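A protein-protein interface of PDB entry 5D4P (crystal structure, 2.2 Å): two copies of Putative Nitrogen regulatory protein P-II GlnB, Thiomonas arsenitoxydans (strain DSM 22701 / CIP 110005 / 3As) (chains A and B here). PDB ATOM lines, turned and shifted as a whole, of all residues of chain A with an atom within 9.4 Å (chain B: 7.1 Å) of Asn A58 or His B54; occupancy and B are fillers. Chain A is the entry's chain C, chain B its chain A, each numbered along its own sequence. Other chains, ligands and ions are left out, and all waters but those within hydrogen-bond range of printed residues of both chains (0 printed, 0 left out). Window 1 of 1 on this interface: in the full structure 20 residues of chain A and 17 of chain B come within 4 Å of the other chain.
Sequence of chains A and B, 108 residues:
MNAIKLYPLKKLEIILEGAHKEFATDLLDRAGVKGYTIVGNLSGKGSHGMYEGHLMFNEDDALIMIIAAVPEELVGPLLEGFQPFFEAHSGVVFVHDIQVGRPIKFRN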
ATOM      1  N   GLY A  18      -1.894   3.754  -3.346  1.00  0.00           N
ATOM      2  CA  GLY A  18      -3.288   3.522  -3.713  1.00  0.00           C
ATOM      3  C   GLY A  18      -4.273   4.426  -2.972  1.00  0.00           C
ATOM      4  O   GLY A  18      -5.365   4.715  -3.462  1.00  0.00           O
ATOM      5  N   LYS A  21      -5.551   7.207  -5.067  1.00  0.00           N
ATOM      6  CA  LYS A  21      -6.054   6.865  -6.385  1.00  0.00           C
ATOM      7  C   LYS A  21      -7.149   7.832  -6.855  1.00  0.00           C
ATOM      8  O   LYS A  21      -7.147   8.251  -8.022  1.00  0.00           O
ATOM      9  CB  LYS A  21      -6.558   5.423  -6.427  1.00  0.00           C
ATOM     10  CG  LYS A  21      -7.216   5.086  -7.766  1.00  0.00           C
ATOM     11  CD  LYS A  21      -7.521   3.612  -7.909  1.00  0.00           C
ATOM     12  CE  LYS A  21      -8.705   3.188  -7.107  1.00  0.00           C
ATOM     13  NZ  LYS A  21      -8.814   1.710  -7.188  1.00  0.00           N
ATOM     14  N   ILE A  38      -5.251   0.775 -14.398  1.00  0.00           N
ATOM     15  CA  ILE A  38      -4.552   0.758 -13.123  1.00  0.00           C
ATOM     16  C   ILE A  38      -3.973  -0.609 -12.859  1.00  0.00           C
ATOM     17  O   ILE A  38      -4.689  -1.608 -12.945  1.00  0.00           O
ATOM     18  CB  ILE A  38      -5.480   1.190 -11.958  1.00  0.00           C
ATOM     19  CG1 ILE A  38      -6.072   2.572 -12.270  1.00  0.00           C
ATOM     20  CG2 ILE A  38      -4.720   1.186 -10.650  1.00  0.00           C
ATOM     21  CD1 ILE A  38      -6.970   3.142 -11.213  1.00  0.00           C
ATOM     22  N   VAL A  39      -2.660  -0.648 -12.622  1.00  0.00           N
ATOM     23  CA  VAL A  39      -1.954  -1.876 -12.232  1.00  0.00           C
ATOM     24  C   VAL A  39      -1.742  -1.881 -10.709  1.00  0.00           C
ATOM     25  O   VAL A  39      -1.027  -1.024 -10.169  1.00  0.00           O
ATOM     26  CB  VAL A  39      -0.595  -1.994 -12.928  1.00  0.00           C
ATOM     27  CG1 VAL A  39       0.051  -3.335 -12.585  1.00  0.00           C
ATOM     28  CG2 VAL A  39      -0.737  -1.835 -14.452  1.00  0.00           C
ATOM     29  N   GLY A  40      -2.350  -2.830 -10.008  1.00  0.00           N
ATOM     30  CA  GLY A  40      -2.245  -2.826  -8.556  1.00  0.00           C
ATOM     31  C   GLY A  40      -1.246  -3.804  -7.979  1.00  0.00           C
ATOM     32  O   GLY A  40      -0.619  -4.579  -8.716  1.00  0.00           O
ATOM     33  N   ASN A  41      -1.117  -3.775  -6.655  1.00  0.00           N
ATOM     34  CA  ASN A  41      -0.274  -4.712  -5.913  1.00  0.00           C
ATOM     35  C   ASN A  41       1.176  -4.698  -6.406  1.00  0.00           C
ATOM     36  O   ASN A  41       1.716  -5.709  -6.851  1.00  0.00           O
ATOM     37  CB  ASN A  41      -0.831  -6.131  -5.980  1.00  0.00           C
ATOM     38  CG  ASN A  41      -0.133  -7.067  -5.010  1.00  0.00           C
ATOM     39  OD1 ASN A  41       0.175  -6.681  -3.879  1.00  0.00           O
ATOM     40  ND2 ASN A  41       0.128  -8.296  -5.446  1.00  0.00           N
ATOM     41  N   LEU A  42       1.798  -3.540  -6.322  1.00  0.00           N
ATOM     42  CA  LEU A  42       3.163  -3.379  -6.765  1.00  0.00           C
ATOM     43  C   LEU A  42       4.095  -3.451  -5.572  1.00  0.00           C
ATOM     44  O   LEU A  42       3.685  -3.262  -4.423  1.00  0.00           O
ATOM     45  CB  LEU A  42       3.370  -2.039  -7.458  1.00  0.00           C
ATOM     46  CG  LEU A  42       2.521  -1.641  -8.648  1.00  0.00           C
ATOM     47  CD1 LEU A  42       2.985  -0.263  -9.090  1.00  0.00           C
ATOM     48  CD2 LEU A  42       2.656  -2.675  -9.760  1.00  0.00           C
ATOM     49  N   GLU A  52       6.101  -3.424  -0.032  1.00  0.00           N
ATOM     50  CA  GLU A  52       6.027  -4.853  -0.312  1.00  0.00           C
ATOM     51  C   GLU A  52       4.670  -5.234  -0.901  1.00  0.00           C
ATOM     52  O   GLU A  52       3.638  -5.093  -0.250  1.00  0.00           O
ATOM     53  CB  GLU A  52       6.298  -5.671   0.955  1.00  0.00           C
ATOM     54  CG  GLU A  52       7.722  -5.560   1.474  1.00  0.00           C
ATOM     55  CD  GLU A  52       8.707  -6.352   0.627  1.00  0.00           C
ATOM     56  OE1 GLU A  52       8.265  -7.163  -0.219  1.00  0.00           O
ATOM     57  OE2 GLU A  52       9.925  -6.155   0.804  1.00  0.00           O
ATOM     58  N   GLY A  53       4.674  -5.753  -2.122  1.00  0.00           N
ATOM     59  CA  GLY A  53       3.439  -6.201  -2.739  1.00  0.00           C
ATOM     60  C   GLY A  53       2.913  -7.407  -1.969  1.00  0.00           C
ATOM     61  O   GLY A  53       3.670  -8.335  -1.656  1.00  0.00           O
ATOM     62  N   HIS A  54       1.622  -7.392  -1.661  1.00  0.00           N
ATOM     63  CA  HIS A  54       0.994  -8.480  -0.921  1.00  0.00           C
ATOM     64  C   HIS A  54       0.955  -9.773  -1.751  1.00  0.00           C
ATOM     65  O   HIS A  54       0.737  -9.736  -2.967  1.00  0.00           O
ATOM     66  CB  HIS A  54      -0.416  -8.070  -0.493  1.00  0.00           C
ATOM     67  CG  HIS A  54      -0.930  -8.831   0.684  1.00  0.00           C
ATOM     68  ND1 HIS A  54      -1.269 -10.166   0.617  1.00  0.00           N
ATOM     69  CD2 HIS A  54      -1.166  -8.445   1.959  1.00  0.00           C
ATOM     70  CE1 HIS A  54      -1.690 -10.569   1.801  1.00  0.00           C
ATOM     71  NE2 HIS A  54      -1.640  -9.545   2.634  1.00  0.00           N
ATOM     72  N   LEU A  55       1.171 -10.914  -1.098  1.00  0.00           N
ATOM     73  CA  LEU A  55       1.172 -12.188  -1.812  1.00  0.00           C
ATOM     74  C   LEU A  55      -0.198 -12.874  -1.902  1.00  0.00           C
ATOM     75  O   LEU A  55      -0.327 -13.888  -2.588  1.00  0.00           O
ATOM     76  CB  LEU A  55       2.169 -13.151  -1.153  1.00  0.00           C
ATOM     77  N   MET A  56      -1.207 -12.343  -1.210  1.00  0.00           N
ATOM     78  CA  MET A  56      -2.547 -12.947  -1.235  1.00  0.00           C
ATOM     79  C   MET A  56      -3.645 -12.081  -1.887  1.00  0.00           C
ATOM     80  O   MET A  56      -4.437 -12.578  -2.692  1.00  0.00           O
ATOM     81  CB  MET A  56      -2.970 -13.338   0.187  1.00  0.00           C
ATOM     82  N   PHE A  57      -3.743 -10.815  -1.479  1.00  0.00           N
ATOM     83  CA  PHE A  57      -4.813  -9.934  -1.963  1.00  0.00           C
ATOM     84  C   PHE A  57      -4.367  -8.493  -2.277  1.00  0.00           C
ATOM     85  O   PHE A  57      -3.198  -8.131  -2.100  1.00  0.00           O
ATOM     86  CB  PHE A  57      -5.963  -9.904  -0.941  1.00  0.00           C
ATOM     87  CG  PHE A  57      -5.639  -9.153   0.329  1.00  0.00           C
ATOM     88  CD1 PHE A  57      -4.937  -9.764   1.356  1.00  0.00           C
ATOM     89  CD2 PHE A  57      -6.051  -7.837   0.496  1.00  0.00           C
ATOM     90  CE1 PHE A  57      -4.644  -9.072   2.519  1.00  0.00           C
ATOM     91  CE2 PHE A  57      -5.761  -7.143   1.659  1.00  0.00           C
ATOM     92  CZ  PHE A  57      -5.057  -7.759   2.669  1.00  0.00           C
ATOM     93  N   ASN A  58      -5.319  -7.674  -2.728  1.00  0.00           N
ATOM     94  CA  ASN A  58      -5.084  -6.243  -2.912  1.00  0.00           C
ATOM     95  C   ASN A  58      -5.477  -5.481  -1.640  1.00  0.00           C
ATOM     96  O   ASN A  58      -6.658  -5.190  -1.422  1.00  0.00           O
ATOM     97  CB  ASN A  58      -5.878  -5.687  -4.101  1.00  0.00           C
ATOM     98  CG  ASN A  58      -5.260  -6.034  -5.442  1.00  0.00           C
ATOM     99  OD1 ASN A  58      -4.164  -5.567  -5.776  1.00  0.00           O
ATOM    100  ND2 ASN A  58      -5.977  -6.833  -6.235  1.00  0.00           N
ATOM    101  N   GLU A  59      -4.493  -5.193  -0.791  1.00  0.00           N
ATOM    102  CA  GLU A  59      -4.723  -4.428   0.435  1.00  0.00           C
ATOM    103  C   GLU A  59      -4.905  -2.934   0.134  1.00  0.00           C
ATOM    104  O   GLU A  59      -4.647  -2.483  -0.991  1.00  0.00           O
ATOM    105  CB  GLU A  59      -3.575  -4.647   1.426  1.00  0.00           C
ATOM    106  CG  GLU A  59      -2.191  -4.506   0.820  1.00  0.00           C
ATOM    107  CD  GLU A  59      -1.083  -4.722   1.832  1.00  0.00           C
ATOM    108  OE1 GLU A  59      -1.402  -4.927   3.027  1.00  0.00           O
ATOM    109  OE2 GLU A  59       0.103  -4.684   1.430  1.00  0.00           O
ATOM    110  N   ASP A  60      -5.346  -2.182   1.142  1.00  0.00           N
ATOM    111  CA  ASP A  60      -5.596  -0.749   1.002  1.00  0.00           C
ATOM    112  C   ASP A  60      -4.323   0.097   0.899  1.00  0.00           C
ATOM    113  O   ASP A  60      -4.292   1.060   0.139  1.00  0.00           O
ATOM    114  CB  ASP A  60      -6.443  -0.256   2.178  1.00  0.00           C
ATOM    115  N   ASP A  61      -3.288  -0.249   1.665  1.00  0.00           N
ATOM    116  CA  ASP A  61      -2.027   0.504   1.634  1.00  0.00           C
ATOM    117  C   ASP A  61      -1.082   0.015   0.548  1.00  0.00           C
ATOM    118  O   ASP A  61       0.113  -0.185   0.777  1.00  0.00           O
ATOM    119  CB  ASP A  61      -1.317   0.452   2.987  1.00  0.00           C
ATOM    120  CG  ASP A  61      -1.839   1.486   3.945  1.00  0.00           C
ATOM    121  OD1 ASP A  61      -2.180   2.588   3.469  1.00  0.00           O
ATOM    122  OD2 ASP A  61      -1.900   1.207   5.159  1.00  0.00           O
ATOM    123  N   ALA A  62      -1.631  -0.174  -0.638  1.00  0.00           N
ATOM    124  CA  ALA A  62      -0.859  -0.672  -1.748  1.00  0.00           C
ATOM    125  C   ALA A  62      -0.148   0.432  -2.525  1.00  0.00           C
ATOM    126  O   ALA A  62      -0.455   1.618  -2.416  1.00  0.00           O
ATOM    127  CB  ALA A  62      -1.761  -1.470  -2.684  1.00  0.00           C
ATOM    128  N   LEU A  63       0.804   0.003  -3.330  1.00  0.00           N
ATOM    129  CA  LEU A  63       1.407   0.857  -4.322  1.00  0.00           C
ATOM    130  C   LEU A  63       0.720   0.498  -5.634  1.00  0.00           C
ATOM    131  O   LEU A  63       0.527  -0.689  -5.927  1.00  0.00           O
ATOM    132  CB  LEU A  63       2.911   0.621  -4.392  1.00  0.00           C
ATOM    133  CG  LEU A  63       3.709   1.593  -5.254  1.00  0.00           C
ATOM    134  CD1 LEU A  63       3.741   2.955  -4.618  1.00  0.00           C
ATOM    135  CD2 LEU A  63       5.122   1.031  -5.498  1.00  0.00           C
ATOM    136  N   ILE A  64       0.361   1.502  -6.426  1.00  0.00           N
ATOM    137  CA  ILE A  64      -0.265   1.254  -7.729  1.00  0.00           C
ATOM    138  C   ILE A  64       0.401   2.050  -8.833  1.00  0.00           C
ATOM    139  O   ILE A  64       1.146   2.995  -8.559  1.00  0.00           O
ATOM    140  CB  ILE A  64      -1.759   1.608  -7.733  1.00  0.00           C
ATOM    141  CG1 ILE A  64      -1.941   3.125  -7.630  1.00  0.00           C
ATOM    142  CG2 ILE A  64      -2.505   0.839  -6.626  1.00  0.00           C
ATOM    143  CD1 ILE A  64      -3.378   3.594  -7.730  1.00  0.00           C
ATOM    144  N   ASN B  41      -4.840  -8.780 -13.105  1.00  0.00           N
ATOM    145  CA  ASN B  41      -5.181  -7.967 -11.925  1.00  0.00           C
ATOM    146  C   ASN B  41      -5.176  -6.477 -12.255  1.00  0.00           C
ATOM    147  O   ASN B  41      -4.447  -5.680 -11.633  1.00  0.00           O
ATOM    148  CB  ASN B  41      -4.192  -8.265 -10.771  1.00  0.00           C
ATOM    149  CG  ASN B  41      -4.573  -7.580  -9.449  1.00  0.00           C
ATOM    150  OD1 ASN B  41      -5.751  -7.485  -9.098  1.00  0.00           O
ATOM    151  ND2 ASN B  41      -3.560  -7.119  -8.704  1.00  0.00           N
ATOM    152  N   LEU B  42      -5.945  -6.123 -13.285  1.00  0.00           N
ATOM    153  CA  LEU B  42      -6.076  -4.730 -13.694  1.00  0.00           C
ATOM    154  C   LEU B  42      -7.472  -4.171 -13.415  1.00  0.00           C
ATOM    155  O   LEU B  42      -8.473  -4.904 -13.403  1.00  0.00           O
ATOM    156  CB  LEU B  42      -5.749  -4.565 -15.182  1.00  0.00           C
ATOM    157  CG  LEU B  42      -4.393  -5.022 -15.725  1.00  0.00           C
ATOM    158  CD1 LEU B  42      -4.321  -4.736 -17.223  1.00  0.00           C
ATOM    159  CD2 LEU B  42      -3.203  -4.370 -14.996  1.00  0.00           C
ATOM    160  N   SER B  43      -7.533  -2.868 -13.185  1.00  0.00           N
ATOM    161  CA  SER B  43      -8.801  -2.159 -13.273  1.00  0.00           C
ATOM    162  C   SER B  43      -8.629  -1.058 -14.318  1.00  0.00           C
ATOM    163  O   SER B  43      -7.529  -0.829 -14.794  1.00  0.00           O
ATOM    164  CB  SER B  43      -9.245  -1.606 -11.908  1.00  0.00           C
ATOM    165  OG  SER B  43      -8.236  -0.800 -11.322  1.00  0.00           O
ATOM    166  N   GLU B  52     -13.634  -3.063 -12.869  1.00  0.00           N
ATOM    167  CA  GLU B  52     -13.170  -3.271 -11.500  1.00  0.00           C
ATOM    168  C   GLU B  52     -12.374  -4.571 -11.337  1.00  0.00           C
ATOM    169  O   GLU B  52     -12.858  -5.666 -11.638  1.00  0.00           O
ATOM    170  CB  GLU B  52     -14.361  -3.258 -10.530  1.00  0.00           C
ATOM    171  N   GLY B  53     -11.127  -4.424 -10.896  1.00  0.00           N
ATOM    172  CA  GLY B  53     -10.256  -5.553 -10.614  1.00  0.00           C
ATOM    173  C   GLY B  53     -10.662  -6.347  -9.383  1.00  0.00           C
ATOM    174  O   GLY B  53     -11.198  -5.791  -8.423  1.00  0.00           O
ATOM    175  N   HIS B  54     -10.403  -7.650  -9.407  1.00  0.00           N
ATOM    176  CA  HIS B  54     -10.700  -8.513  -8.271  1.00  0.00           C
ATOM    177  C   HIS B  54      -9.783  -8.187  -7.090  1.00  0.00           C
ATOM    178  O   HIS B  54      -8.692  -7.631  -7.270  1.00  0.00           O
ATOM    179  CB  HIS B  54     -10.551  -9.986  -8.660  1.00  0.00           C
ATOM    180  N   LEU B  55     -10.219  -8.542  -5.882  1.00  0.00           N
ATOM    181  CA  LEU B  55      -9.410  -8.287  -4.696  1.00  0.00           C
ATOM    182  C   LEU B  55      -8.450  -9.442  -4.387  1.00  0.00           C
ATOM    183  O   LEU B  55      -7.534  -9.288  -3.584  1.00  0.00           O
ATOM    184  CB  LEU B  55     -10.321  -8.036  -3.483  1.00  0.00           C
ATOM    185  N   MET B  56      -8.610 -10.566  -5.082  1.00  0.00           N
ATOM    186  CA  MET B  56      -7.764 -11.735  -4.851  1.00  0.00           C
ATOM    187  C   MET B  56      -6.800 -11.993  -6.015  1.00  0.00           C
ATOM    188  O   MET B  56      -6.682 -13.122  -6.499  1.00  0.00           O
ATOM    189  CB  MET B  56      -8.629 -12.973  -4.605  1.00  0.00           C
ATOM    190  CG  MET B  56      -9.506 -12.891  -3.368  1.00  0.00           C
ATOM    191  SD  MET B  56      -8.598 -12.921  -1.810  1.00  0.00           S
ATOM    192  CE  MET B  56      -8.208 -14.658  -1.652  1.00  0.00           C
ATOM    193  N   ASP B  60     -10.304 -15.071 -13.291  1.00  0.00           N
ATOM    194  CA  ASP B  60     -10.204 -14.094 -12.208  1.00  0.00           C
ATOM    195  C   ASP B  60      -9.888 -12.713 -12.769  1.00  0.00           C
ATOM    196  O   ASP B  60     -10.372 -11.696 -12.260  1.00  0.00           O
ATOM    197  CB  ASP B  60      -9.137 -14.512 -11.190  1.00  0.00           C
ATOM    198  N   ASP B  61      -9.063 -12.698 -13.817  1.00  0.00           N
ATOM    199  CA  ASP B  61      -8.610 -11.471 -14.475  1.00  0.00           C
ATOM    200  C   ASP B  61      -9.592 -10.995 -15.543  1.00  0.00           C
ATOM    201  O   ASP B  61      -9.663 -11.575 -16.628  1.00  0.00           O
ATOM    202  CB  ASP B  61      -7.225 -11.694 -15.098  1.00  0.00           C
ATOM    203  CG  ASP B  61      -6.106 -11.606 -14.074  1.00  0.00           C
ATOM    204  OD1 ASP B  61      -6.205 -10.766 -13.155  1.00  0.00           O
ATOM    205  OD2 ASP B  61      -5.147 -12.404 -14.166  1.00  0.00           O
ATOM    206  N   ALA B  62     -10.321  -9.925 -15.245  1.00  0.00           N
ATOM    207  CA  ALA B  62     -11.342  -9.415 -16.155  1.00  0.00           C
ATOM    208  C   ALA B  62     -10.725  -8.531 -17.235  1.00  0.00           C
ATOM    209  O   ALA B  62     -11.121  -8.601 -18.395  1.00  0.00           O
ATOM    210  CB  ALA B  62     -12.413  -8.635 -15.379  1.00  0.00           C
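Among the printed residues, merely in contact across the chains: Ile A38 with Leu B42 (3.5 Å), Val A39 with Leu B42 (3.6 Å), Gly A40 with Asn B41 (3.9 Å), Asn A41 with Asn B41 (3.98 Å) and Phe A57 with Leu B55 (3.1 Å).
A ring nitrogen (ND1) of His A54 lies within hydrogen-bond range of the backbone NH of Phe A57.
The side-chain amide oxygen (OD1) of Asn A41 lies within hydrogen-bond range of the backbone NH (N) of His A54 (2.7 Å).
OD1 of Asn B41 sits close to O of His B54, at 3.5 Å.
N of Asn B41 is in hydrogen-bond range of OD1 of Asp B61 (2.4 Å).
The side-chain amide oxygen (OD1) of Asn B41 lies within hydrogen-bond range of the side-chain amide nitrogen (ND2) of Asn A58 (2.9 Å).
The side-chain amide nitrogen of Asn A58 sits at hydrogen-bond distance from the backbone carbonyl oxygen of His B54 (3.0 Å).
The backbone carbonyl oxygen (O) of Ser B43 is in hydrogen-bond range of the backbone NH (N) of Ile A38.
The backbone NH (N) of Asn A58 sits at hydrogen-bond distance from the backbone carbonyl oxygen (O) of Leu B55.
Of the 11 printed residues of chain B, 5 touch a printed residue of chain A.
Hydrophobic or aromatic side chains of chain B that line the printed part of chain A: Leu B42.
Among the printed residues, no Asp or Glu carboxylate lies within 4 Å of a Lys or Arg side-chain nitrogen of the other chain.
Of chain B, only Asn B41, His B54 and Leu B55 come within 4 Å of Asn A58.
Leu B55 touches two residues of chain A.
Printed residues of chain A within 4 Å of Leu B42: Ile A38 and Val A39.
Of the printed residues of chain B, Asn A41 touches Asn B41 (3.98 Å).
Of the printed residues of chain A, Asn B41 touches Gly A40 (3.9 Å), Asn A41 (3.98 Å) and Asn A58 (2.9 Å).
Printed residues of chain A within 4 Å of Ser B43: Ile A38.
Of the printed residues of chain B, Val A39 touches Leu B42.
Met A56 touches none of the printed residues of chain B.
Leu A42 touches none of the printed residues of chain B.
The nearest residue of chain B that does not touch Asn A58 is Met B56 (4.7 Å).
Asn A41 touches its own counterpart, Asn B41.
Positions printed for both chains: 41, 42, 52, 53, 54, 55, 56, 60, 61 and 62.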
